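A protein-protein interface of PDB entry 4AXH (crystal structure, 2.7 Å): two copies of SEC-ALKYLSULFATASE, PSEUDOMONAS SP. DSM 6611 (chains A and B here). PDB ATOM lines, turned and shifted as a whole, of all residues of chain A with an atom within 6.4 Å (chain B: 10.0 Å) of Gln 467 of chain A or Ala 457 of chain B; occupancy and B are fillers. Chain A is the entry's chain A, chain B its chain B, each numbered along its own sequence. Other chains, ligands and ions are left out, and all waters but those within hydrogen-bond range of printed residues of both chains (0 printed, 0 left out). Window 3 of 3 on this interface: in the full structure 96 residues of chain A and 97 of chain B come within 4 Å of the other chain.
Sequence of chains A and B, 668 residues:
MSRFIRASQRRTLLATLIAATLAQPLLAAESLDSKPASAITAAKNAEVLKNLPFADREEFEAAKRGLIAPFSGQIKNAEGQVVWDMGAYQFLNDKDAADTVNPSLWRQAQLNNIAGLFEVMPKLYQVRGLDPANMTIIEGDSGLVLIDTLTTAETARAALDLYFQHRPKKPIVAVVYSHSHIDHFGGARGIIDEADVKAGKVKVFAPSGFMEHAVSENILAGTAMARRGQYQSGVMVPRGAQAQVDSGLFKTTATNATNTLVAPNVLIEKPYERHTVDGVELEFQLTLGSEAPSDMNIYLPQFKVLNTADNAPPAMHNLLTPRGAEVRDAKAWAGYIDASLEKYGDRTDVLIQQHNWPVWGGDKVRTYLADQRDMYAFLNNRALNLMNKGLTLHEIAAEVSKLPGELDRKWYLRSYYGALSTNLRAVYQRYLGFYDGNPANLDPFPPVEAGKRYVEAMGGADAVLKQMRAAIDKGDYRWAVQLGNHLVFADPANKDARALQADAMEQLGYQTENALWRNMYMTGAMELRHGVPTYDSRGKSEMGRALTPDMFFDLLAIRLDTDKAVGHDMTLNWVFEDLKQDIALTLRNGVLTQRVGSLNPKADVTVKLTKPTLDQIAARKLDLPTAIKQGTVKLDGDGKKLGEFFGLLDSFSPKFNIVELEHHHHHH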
ATOM      1  N   ALA A 457     -17.822  -4.608   8.983  1.00  0.00           N
ATOM      2  CA  ALA A 457     -17.199  -5.899   9.281  1.00  0.00           C
ATOM      3  C   ALA A 457     -17.975  -6.684  10.324  1.00  0.00           C
ATOM      4  O   ALA A 457     -17.968  -7.912  10.295  1.00  0.00           O
ATOM      5  CB  ALA A 457     -15.769  -5.692   9.750  1.00  0.00           C
ATOM      6  N   MET A 458     -18.664  -5.978  11.226  1.00  0.00           N
ATOM      7  CA  MET A 458     -19.430  -6.589  12.304  1.00  0.00           C
ATOM      8  C   MET A 458     -20.887  -6.923  11.962  1.00  0.00           C
ATOM      9  O   MET A 458     -21.609  -7.450  12.810  1.00  0.00           O
ATOM     10  CB  MET A 458     -19.291  -5.770  13.597  1.00  0.00           C
ATOM     11  CG  MET A 458     -17.900  -5.872  14.227  1.00  0.00           C
ATOM     12  SD  MET A 458     -17.708  -5.013  15.810  1.00  0.00           S
ATOM     13  CE  MET A 458     -17.429  -3.370  15.269  1.00  0.00           C
ATOM     14  N   GLY A 459     -21.288  -6.662  10.720  1.00  0.00           N
ATOM     15  CA  GLY A 459     -22.625  -6.978  10.217  1.00  0.00           C
ATOM     16  C   GLY A 459     -23.568  -5.827   9.923  1.00  0.00           C
ATOM     17  O   GLY A 459     -24.639  -6.038   9.346  1.00  0.00           O
ATOM     18  N   ASP A 462     -27.482  -2.388  12.839  1.00  0.00           N
ATOM     19  CA  ASP A 462     -28.413  -3.194  13.623  1.00  0.00           C
ATOM     20  C   ASP A 462     -27.680  -4.342  14.324  1.00  0.00           C
ATOM     21  O   ASP A 462     -27.945  -4.606  15.499  1.00  0.00           O
ATOM     22  CB  ASP A 462     -29.557  -3.723  12.736  1.00  0.00           C
ATOM     23  CG  ASP A 462     -30.598  -2.684  12.330  1.00  0.00           C
ATOM     24  OD1 ASP A 462     -31.187  -2.037  13.235  1.00  0.00           O
ATOM     25  OD2 ASP A 462     -30.871  -2.563  11.116  1.00  0.00           O
ATOM     26  N   ALA A 463     -26.747  -5.007  13.605  1.00  0.00           N
ATOM     27  CA  ALA A 463     -25.971  -6.135  14.140  1.00  0.00           C
ATOM     28  C   ALA A 463     -25.083  -5.688  15.294  1.00  0.00           C
ATOM     29  O   ALA A 463     -25.078  -6.337  16.343  1.00  0.00           O
ATOM     30  CB  ALA A 463     -25.137  -6.776  13.045  1.00  0.00           C
ATOM     31  N   VAL A 464     -24.393  -4.537  15.129  1.00  0.00           N
ATOM     32  CA  VAL A 464     -23.543  -3.968  16.169  1.00  0.00           C
ATOM     33  C   VAL A 464     -24.390  -3.567  17.395  1.00  0.00           C
ATOM     34  O   VAL A 464     -23.953  -3.791  18.518  1.00  0.00           O
ATOM     35  CB  VAL A 464     -22.548  -2.875  15.668  1.00  0.00           C
ATOM     36  CG1 VAL A 464     -21.758  -3.352  14.459  1.00  0.00           C
ATOM     37  CG2 VAL A 464     -23.243  -1.567  15.344  1.00  0.00           C
ATOM     38  N   LEU A 465     -25.634  -3.077  17.164  1.00  0.00           N
ATOM     39  CA  LEU A 465     -26.604  -2.681  18.196  1.00  0.00           C
ATOM     40  C   LEU A 465     -27.108  -3.881  19.032  1.00  0.00           C
ATOM     41  O   LEU A 465     -27.333  -3.736  20.236  1.00  0.00           O
ATOM     42  CB  LEU A 465     -27.801  -1.929  17.571  1.00  0.00           C
ATOM     43  CG  LEU A 465     -27.716  -0.390  17.488  1.00  0.00           C
ATOM     44  CD1 LEU A 465     -28.504   0.137  16.318  1.00  0.00           C
ATOM     45  CD2 LEU A 465     -28.249   0.271  18.744  1.00  0.00           C
ATOM     46  N   LYS A 466     -27.298  -5.051  18.391  1.00  0.00           N
ATOM     47  CA  LYS A 466     -27.747  -6.291  19.043  1.00  0.00           C
ATOM     48  C   LYS A 466     -26.617  -6.814  19.935  1.00  0.00           C
ATOM     49  O   LYS A 466     -26.872  -7.245  21.058  1.00  0.00           O
ATOM     50  CB  LYS A 466     -28.115  -7.350  17.975  1.00  0.00           C
ATOM     51  CG  LYS A 466     -29.216  -8.332  18.393  1.00  0.00           C
ATOM     52  CD  LYS A 466     -28.688  -9.592  19.077  1.00  0.00           C
ATOM     53  CE  LYS A 466     -29.808 -10.379  19.709  1.00  0.00           C
ATOM     54  NZ  LYS A 466     -29.304 -11.341  20.724  1.00  0.00           N
ATOM     55  N   GLN A 467     -25.372  -6.758  19.413  1.00  0.00           N
ATOM     56  CA  GLN A 467     -24.135  -7.141  20.088  1.00  0.00           C
ATOM     57  C   GLN A 467     -23.857  -6.228  21.279  1.00  0.00           C
ATOM     58  O   GLN A 467     -23.408  -6.701  22.322  1.00  0.00           O
ATOM     59  CB  GLN A 467     -22.961  -7.062  19.121  1.00  0.00           C
ATOM     60  CG  GLN A 467     -22.932  -8.186  18.115  1.00  0.00           C
ATOM     61  CD  GLN A 467     -21.566  -8.294  17.523  1.00  0.00           C
ATOM     62  OE1 GLN A 467     -20.564  -8.361  18.243  1.00  0.00           O
ATOM     63  NE2 GLN A 467     -21.499  -8.308  16.200  1.00  0.00           N
ATOM     64  N   MET A 468     -24.111  -4.928  21.109  1.00  0.00           N
ATOM     65  CA  MET A 468     -23.961  -3.902  22.126  1.00  0.00           C
ATOM     66  C   MET A 468     -24.934  -4.214  23.273  1.00  0.00           C
ATOM     67  O   MET A 468     -24.538  -4.150  24.444  1.00  0.00           O
ATOM     68  CB  MET A 468     -24.326  -2.540  21.525  1.00  0.00           C
ATOM     69  CG  MET A 468     -23.298  -1.458  21.722  1.00  0.00           C
ATOM     70  SD  MET A 468     -23.927   0.194  21.260  1.00  0.00           S
ATOM     71  CE  MET A 468     -23.882   0.066  19.458  1.00  0.00           C
ATOM     72  N   ARG A 469     -26.205  -4.569  22.933  1.00  0.00           N
ATOM     73  CA  ARG A 469     -27.247  -4.894  23.912  1.00  0.00           C
ATOM     74  C   ARG A 469     -26.870  -6.130  24.730  1.00  0.00           C
ATOM     75  O   ARG A 469     -27.103  -6.159  25.944  1.00  0.00           O
ATOM     76  CB  ARG A 469     -28.633  -5.029  23.253  1.00  0.00           C
ATOM     77  CG  ARG A 469     -29.328  -3.675  23.030  1.00  0.00           C
ATOM     78  CD  ARG A 469     -30.842  -3.759  22.868  1.00  0.00           C
ATOM     79  NE  ARG A 469     -31.508  -2.480  23.153  1.00  0.00           N
ATOM     80  CZ  ARG A 469     -31.770  -1.535  22.249  1.00  0.00           C
ATOM     81  NH1 ARG A 469     -31.420  -1.705  20.976  1.00  0.00           N
ATOM     82  NH2 ARG A 469     -32.376  -0.408  22.612  1.00  0.00           N
ATOM     83  N   ALA A 470     -26.223  -7.118  24.069  1.00  0.00           N
ATOM     84  CA  ALA A 470     -25.768  -8.368  24.684  1.00  0.00           C
ATOM     85  C   ALA A 470     -24.702  -8.073  25.728  1.00  0.00           C
ATOM     86  O   ALA A 470     -24.803  -8.576  26.848  1.00  0.00           O
ATOM     87  CB  ALA A 470     -25.224  -9.317  23.624  1.00  0.00           C
ATOM     88  N   ALA A 471     -23.718  -7.203  25.371  1.00  0.00           N
ATOM     89  CA  ALA A 471     -22.613  -6.753  26.227  1.00  0.00           C
ATOM     90  C   ALA A 471     -23.097  -6.085  27.504  1.00  0.00           C
ATOM     91  O   ALA A 471     -22.515  -6.340  28.553  1.00  0.00           O
ATOM     92  CB  ALA A 471     -21.687  -5.824  25.462  1.00  0.00           C
ATOM     93  N   ILE A 472     -24.171  -5.267  27.438  1.00  0.00           N
ATOM     94  CA  ILE A 472     -24.692  -4.605  28.633  1.00  0.00           C
ATOM     95  C   ILE A 472     -25.367  -5.612  29.575  1.00  0.00           C
ATOM     96  O   ILE A 472     -25.114  -5.586  30.781  1.00  0.00           O
ATOM     97  CB  ILE A 472     -25.493  -3.280  28.373  1.00  0.00           C
ATOM     98  CG1 ILE A 472     -26.983  -3.499  28.134  1.00  0.00           C
ATOM     99  CG2 ILE A 472     -24.863  -2.382  27.300  1.00  0.00           C
ATOM    100  CD1 ILE A 472     -27.864  -3.151  29.340  1.00  0.00           C
ATOM    101  N   TRP A 479     -16.631  -3.560  26.843  1.00  0.00           N
ATOM    102  CA  TRP A 479     -16.723  -3.967  25.445  1.00  0.00           C
ATOM    103  C   TRP A 479     -17.872  -3.237  24.764  1.00  0.00           C
ATOM    104  O   TRP A 479     -17.704  -2.765  23.642  1.00  0.00           O
ATOM    105  CB  TRP A 479     -16.800  -5.487  25.293  1.00  0.00           C
ATOM    106  CG  TRP A 479     -16.935  -5.951  23.871  1.00  0.00           C
ATOM    107  CD1 TRP A 479     -18.008  -6.590  23.317  1.00  0.00           C
ATOM    108  CD2 TRP A 479     -15.991  -5.753  22.802  1.00  0.00           C
ATOM    109  NE1 TRP A 479     -17.787  -6.809  21.972  1.00  0.00           N
ATOM    110  CE2 TRP A 479     -16.550  -6.325  21.637  1.00  0.00           C
ATOM    111  CE3 TRP A 479     -14.711  -5.182  22.727  1.00  0.00           C
ATOM    112  CZ2 TRP A 479     -15.879  -6.345  20.417  1.00  0.00           C
ATOM    113  CZ3 TRP A 479     -14.057  -5.177  21.509  1.00  0.00           C
ATOM    114  CH2 TRP A 479     -14.641  -5.749  20.369  1.00  0.00           C
ATOM    115  N   ALA A 480     -18.999  -3.066  25.471  1.00  0.00           N
ATOM    116  CA  ALA A 480     -20.139  -2.310  24.976  1.00  0.00           C
ATOM    117  C   ALA A 480     -19.720  -0.911  24.457  1.00  0.00           C
ATOM    118  O   ALA A 480     -20.066  -0.587  23.325  1.00  0.00           O
ATOM    119  CB  ALA A 480     -21.184  -2.169  26.062  1.00  0.00           C
ATOM    120  N   LEU A 483     -17.873  -0.929  20.993  1.00  0.00           N
ATOM    121  CA  LEU A 483     -18.805  -1.102  19.867  1.00  0.00           C
ATOM    122  C   LEU A 483     -19.548   0.206  19.603  1.00  0.00           C
ATOM    123  O   LEU A 483     -19.554   0.687  18.464  1.00  0.00           O
ATOM    124  CB  LEU A 483     -19.829  -2.232  20.116  1.00  0.00           C
ATOM    125  CG  LEU A 483     -19.332  -3.685  20.307  1.00  0.00           C
ATOM    126  CD1 LEU A 483     -20.402  -4.668  19.980  1.00  0.00           C
ATOM    127  CD2 LEU A 483     -18.171  -4.027  19.390  1.00  0.00           C
ATOM    128  N   GLU B 449      -6.576  -9.590  24.006  1.00  0.00           N
ATOM    129  CA  GLU B 449      -7.951  -9.510  24.493  1.00  0.00           C
ATOM    130  C   GLU B 449      -8.877  -8.786  23.517  1.00  0.00           C
ATOM    131  O   GLU B 449      -9.989  -9.249  23.279  1.00  0.00           O
ATOM    132  CB  GLU B 449      -7.999  -8.866  25.884  1.00  0.00           C
ATOM    133  CG  GLU B 449      -8.199  -9.873  27.000  1.00  0.00           C
ATOM    134  CD  GLU B 449      -9.656 -10.084  27.359  1.00  0.00           C
ATOM    135  OE1 GLU B 449     -10.189  -9.260  28.136  1.00  0.00           O
ATOM    136  OE2 GLU B 449     -10.269 -11.057  26.860  1.00  0.00           O
ATOM    137  N   ALA B 450      -8.421  -7.668  22.947  1.00  0.00           N
ATOM    138  CA  ALA B 450      -9.209  -6.903  21.984  1.00  0.00           C
ATOM    139  C   ALA B 450      -9.436  -7.748  20.711  1.00  0.00           C
ATOM    140  O   ALA B 450     -10.578  -7.856  20.237  1.00  0.00           O
ATOM    141  CB  ALA B 450      -8.498  -5.601  21.649  1.00  0.00           C
ATOM    142  N   GLY B 451      -8.359  -8.392  20.236  1.00  0.00           N
ATOM    143  CA  GLY B 451      -8.356  -9.265  19.063  1.00  0.00           C
ATOM    144  C   GLY B 451      -9.385 -10.378  19.102  1.00  0.00           C
ATOM    145  O   GLY B 451     -10.058 -10.627  18.102  1.00  0.00           O
ATOM    146  N   LYS B 452      -9.531 -11.030  20.268  1.00  0.00           N
ATOM    147  CA  LYS B 452     -10.485 -12.113  20.515  1.00  0.00           C
ATOM    148  C   LYS B 452     -11.940 -11.628  20.407  1.00  0.00           C
ATOM    149  O   LYS B 452     -12.731 -12.249  19.679  1.00  0.00           O
ATOM    150  CB  LYS B 452     -10.213 -12.768  21.890  1.00  0.00           C
ATOM    151  CG  LYS B 452      -9.243 -13.953  21.860  1.00  0.00           C
ATOM    152  CD  LYS B 452     -10.001 -15.295  21.838  1.00  0.00           C
ATOM    153  CE  LYS B 452      -9.164 -16.514  21.518  1.00  0.00           C
ATOM    154  NZ  LYS B 452      -8.086 -16.745  22.520  1.00  0.00           N
ATOM    155  N   ARG B 453     -12.273 -10.505  21.116  1.00  0.00           N
ATOM    156  CA  ARG B 453     -13.632  -9.971  21.099  1.00  0.00           C
ATOM    157  C   ARG B 453     -14.014  -9.335  19.781  1.00  0.00           C
ATOM    158  O   ARG B 453     -15.182  -9.437  19.407  1.00  0.00           O
ATOM    159  CB  ARG B 453     -13.988  -9.132  22.345  1.00  0.00           C
ATOM    160  CG  ARG B 453     -14.747  -9.927  23.432  1.00  0.00           C
ATOM    161  CD  ARG B 453     -13.846 -10.916  24.175  1.00  0.00           C
ATOM    162  NE  ARG B 453     -14.556 -11.693  25.195  1.00  0.00           N
ATOM    163  CZ  ARG B 453     -14.018 -12.693  25.890  1.00  0.00           C
ATOM    164  NH1 ARG B 453     -12.760 -13.057  25.677  1.00  0.00           N
ATOM    165  NH2 ARG B 453     -14.736 -13.336  26.801  1.00  0.00           N
ATOM    166  N   TYR B 454     -13.045  -8.757  19.036  1.00  0.00           N
ATOM    167  CA  TYR B 454     -13.315  -8.206  17.708  1.00  0.00           C
ATOM    168  C   TYR B 454     -13.590  -9.326  16.685  1.00  0.00           C
ATOM    169  O   TYR B 454     -14.588  -9.240  15.969  1.00  0.00           O
ATOM    170  CB  TYR B 454     -12.188  -7.280  17.223  1.00  0.00           C
ATOM    171  CG  TYR B 454     -12.325  -5.845  17.678  1.00  0.00           C
ATOM    172  CD1 TYR B 454     -13.262  -4.994  17.099  1.00  0.00           C
ATOM    173  CD2 TYR B 454     -11.467  -5.313  18.629  1.00  0.00           C
ATOM    174  CE1 TYR B 454     -13.369  -3.661  17.489  1.00  0.00           C
ATOM    175  CE2 TYR B 454     -11.565  -3.984  19.028  1.00  0.00           C
ATOM    176  CZ  TYR B 454     -12.516  -3.160  18.452  1.00  0.00           C
ATOM    177  OH  TYR B 454     -12.607  -1.850  18.849  1.00  0.00           O
ATOM    178  N   VAL B 455     -12.732 -10.387  16.644  1.00  0.00           N
ATOM    179  CA  VAL B 455     -12.869 -11.561  15.762  1.00  0.00           C
ATOM    180  C   VAL B 455     -14.256 -12.202  15.946  1.00  0.00           C
ATOM    181  O   VAL B 455     -14.941 -12.480  14.957  1.00  0.00           O
ATOM    182  CB  VAL B 455     -11.684 -12.566  15.919  1.00  0.00           C
ATOM    183  CG1 VAL B 455     -11.984 -13.924  15.279  1.00  0.00           C
ATOM    184  CG2 VAL B 455     -10.398 -11.978  15.344  1.00  0.00           C
ATOM    185  N   GLU B 456     -14.678 -12.362  17.210  1.00  0.00           N
ATOM    186  CA  GLU B 456     -15.994 -12.866  17.607  1.00  0.00           C
ATOM    187  C   GLU B 456     -17.084 -11.935  17.022  1.00  0.00           C
ATOM    188  O   GLU B 456     -17.968 -12.408  16.311  1.00  0.00           O
ATOM    189  CB  GLU B 456     -16.072 -12.944  19.155  1.00  0.00           C
ATOM    190  CG  GLU B 456     -17.456 -13.185  19.746  1.00  0.00           C
ATOM    191  CD  GLU B 456     -17.736 -12.434  21.036  1.00  0.00           C
ATOM    192  OE1 GLU B 456     -17.698 -11.180  21.034  1.00  0.00           O
ATOM    193  OE2 GLU B 456     -18.042 -13.109  22.043  1.00  0.00           O
ATOM    194  N   ALA B 457     -16.973 -10.609  17.274  1.00  0.00           N
ATOM    195  CA  ALA B 457     -17.904  -9.588  16.795  1.00  0.00           C
ATOM    196  C   ALA B 457     -17.977  -9.543  15.275  1.00  0.00           C
ATOM    197  O   ALA B 457     -19.021  -9.211  14.719  1.00  0.00           O
ATOM    198  CB  ALA B 457     -17.502  -8.231  17.334  1.00  0.00           C
ATOM    199  N   MET B 458     -16.883  -9.907  14.608  1.00  0.00           N
ATOM    200  CA  MET B 458     -16.804  -9.900  13.157  1.00  0.00           C
ATOM    201  C   MET B 458     -17.279 -11.212  12.459  1.00  0.00           C
ATOM    202  O   MET B 458     -17.266 -11.288  11.219  1.00  0.00           O
ATOM    203  CB  MET B 458     -15.415  -9.444  12.700  1.00  0.00           C
ATOM    204  CG  MET B 458     -15.172  -7.972  12.926  1.00  0.00           C
ATOM    205  SD  MET B 458     -13.593  -7.355  12.285  1.00  0.00           S
ATOM    206  CE  MET B 458     -12.529  -7.795  13.595  1.00  0.00           C
ATOM    207  N   GLY B 459     -17.730 -12.192  13.251  1.00  0.00           N
ATOM    208  CA  GLY B 459     -18.257 -13.459  12.748  1.00  0.00           C
ATOM    209  C   GLY B 459     -17.429 -14.714  12.992  1.00  0.00           C
ATOM    210  O   GLY B 459     -17.905 -15.831  12.742  1.00  0.00           O
ATOM    211  N   GLY B 460     -16.194 -14.543  13.457  1.00  0.00           N
ATOM    212  CA  GLY B 460     -15.308 -15.666  13.716  1.00  0.00           C
ATOM    213  C   GLY B 460     -14.121 -15.693  12.785  1.00  0.00           C
ATOM    214  O   GLY B 460     -14.101 -14.998  11.758  1.00  0.00           O
ATOM    215  N   ALA B 461     -13.120 -16.513  13.160  1.00  0.00           N
ATOM    216  CA  ALA B 461     -11.841 -16.695  12.468  1.00  0.00           C
ATOM    217  C   ALA B 461     -11.951 -16.819  10.944  1.00  0.00           C
ATOM    218  O   ALA B 461     -11.215 -16.143  10.230  1.00  0.00           O
ATOM    219  CB  ALA B 461     -11.096 -17.888  13.054  1.00  0.00           C
ATOM    220  N   ALA B 463     -14.683 -15.950   9.070  1.00  0.00           N
ATOM    221  CA  ALA B 463     -15.347 -14.742   8.584  1.00  0.00           C
ATOM    222  C   ALA B 463     -14.358 -13.594   8.438  1.00  0.00           C
ATOM    223  O   ALA B 463     -14.330 -12.937   7.391  1.00  0.00           O
ATOM    224  CB  ALA B 463     -16.495 -14.362   9.509  1.00  0.00           C
ATOM    225  N   VAL B 464     -13.499 -13.404   9.460  1.00  0.00           N
ATOM    226  CA  VAL B 464     -12.470 -12.366   9.439  1.00  0.00           C
ATOM    227  C   VAL B 464     -11.448 -12.634   8.307  1.00  0.00           C
ATOM    228  O   VAL B 464     -11.023 -11.692   7.636  1.00  0.00           O
ATOM    229  CB  VAL B 464     -11.838 -12.056  10.839  1.00  0.00           C
ATOM    230  CG1 VAL B 464     -12.907 -11.813  11.895  1.00  0.00           C
ATOM    231  CG2 VAL B 464     -10.909 -13.160  11.306  1.00  0.00           C
ATOM    232  N   GLN B 467     -12.990 -11.671   4.874  1.00  0.00           N
ATOM    233  CA  GLN B 467     -12.976 -10.212   4.862  1.00  0.00           C
ATOM    234  C   GLN B 467     -11.572  -9.687   4.584  1.00  0.00           C
ATOM    235  O   GLN B 467     -11.410  -8.704   3.858  1.00  0.00           O
ATOM    236  CB  GLN B 467     -13.457  -9.684   6.211  1.00  0.00           C
ATOM    237  CG  GLN B 467     -14.947  -9.806   6.427  1.00  0.00           C
ATOM    238  CD  GLN B 467     -15.379  -8.886   7.521  1.00  0.00           C
ATOM    239  OE1 GLN B 467     -15.048  -7.694   7.519  1.00  0.00           O
ATOM    240  NE2 GLN B 467     -16.119  -9.423   8.485  1.00  0.00           N
ATOM    241  N   HIS B 486      -5.889  -8.534  14.625  1.00  0.00           N
ATOM    242  CA  HIS B 486      -6.887  -9.026  15.566  1.00  0.00           C
ATOM    243  C   HIS B 486      -6.902 -10.538  15.599  1.00  0.00           C
ATOM    244  O   HIS B 486      -6.966 -11.117  16.688  1.00  0.00           O
ATOM    245  CB  HIS B 486      -8.287  -8.483  15.249  1.00  0.00           C
ATOM    246  CG  HIS B 486      -8.475  -7.056  15.651  1.00  0.00           C
ATOM    247  ND1 HIS B 486      -8.689  -6.526  16.876  1.00  0.00           N
ATOM    248  CD2 HIS B 486      -8.407  -6.029  14.724  1.00  0.00           C
ATOM    249  CE1 HIS B 486      -8.779  -5.166  16.704  1.00  0.00           C
ATOM    250  NE2 HIS B 486      -8.589  -4.917  15.410  1.00  0.00           N
ATOM    251  N   ALA B 490      -5.500 -13.108  18.607  1.00  0.00           N
ATOM    252  CA  ALA B 490      -6.539 -13.965  19.170  1.00  0.00           C
ATOM    253  C   ALA B 490      -6.087 -15.426  19.127  1.00  0.00           C
ATOM    254  O   ALA B 490      -6.392 -16.197  20.038  1.00  0.00           O
ATOM    255  CB  ALA B 490      -7.827 -13.805  18.385  1.00  0.00           C
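Ala 457 of chain A touches Met 458 of chain B. O of Ala 457 of chain B touches CG of Met 458 of chain A, 3.6 Å away. Met 458 of chain B touches Met 458 of chain A. CZ2 of Trp 479 of chain A touches O of Arg 453 of chain B (3.3 Å). Trp 479 of chain A touches Tyr 454 of chain B. Ala 457 of chain B touches Trp 479 of chain A (CB to CZ2, 3.96 Å).
NE2 of Gln 467 of chain B lies within hydrogen-bond range of O of Ala 457 of chain A (3.0 Å). NE2 of Gln 467 of chain A lies within hydrogen-bond range of O of Ala 457 of chain B (3.0 Å).
Hydrophobic or aromatic side chains of chain A within 4 Å of the printed part of chain B: Ala 457, Met 458 and Trp 479. Of the 18 printed residues of chain B, 5 touch a printed residue of chain A. Hydrophobic or aromatic side chains of chain B within 4 Å of the printed part of chain A: Tyr 454, Ala 457 and Met 458.
O of Met 458 of chain A is in hydrogen-bond range of NE2 of Gln 467 of chain A, at 3.5 Å. The guanidinium group of Arg 453 of chain B is in salt-bridge range of the side-chain carboxylate of Glu 449 of chain B, at 3.4 Å.
Ala 457 of chain A touches Met 458 of chain B, and with the chains exchanged Met 458 of chain A touches Ala 457 of chain B. Ala 457 of chain A touches Gln 467 of chain B, and with the chains exchanged Gln 467 of chain A touches Ala 457 of chain B. Met 458 of chain B touches its own counterpart, Met 458 of chain A. Of the 8 pairs that touch across the chains among the printed residues, 5 have their exchanged pair printed and touching as well.
Printed residues of chain A within 4 Å of Ala 457 of chain B: Met 458, Gln 467 and Trp 479. Of chain B, only Ala 457 (3.6 Å) and Met 458 (3.7 Å) come within 4 Å of Met 458 of chain A. Printed residues of chain B within 4 Å of Ala 457 of chain A: Met 458 and Gln 467. Printed residues of chain A within 4 Å of Met 458 of chain B: Ala 457 (3.6 Å) and Met 458 (3.7 Å). Ala 480 of chain A touches none of the printed residues of chain B. Glu 456 of chain B touches none of the printed residues of chain A. The nearest printed residue of chain A that does not touch Ala 457 of chain B is Leu 483 of chain A (4.7 Å). The nearest printed residue of chain A that does not touch Arg 453 of chain B is Gln 467 of chain A (5.6 Å).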
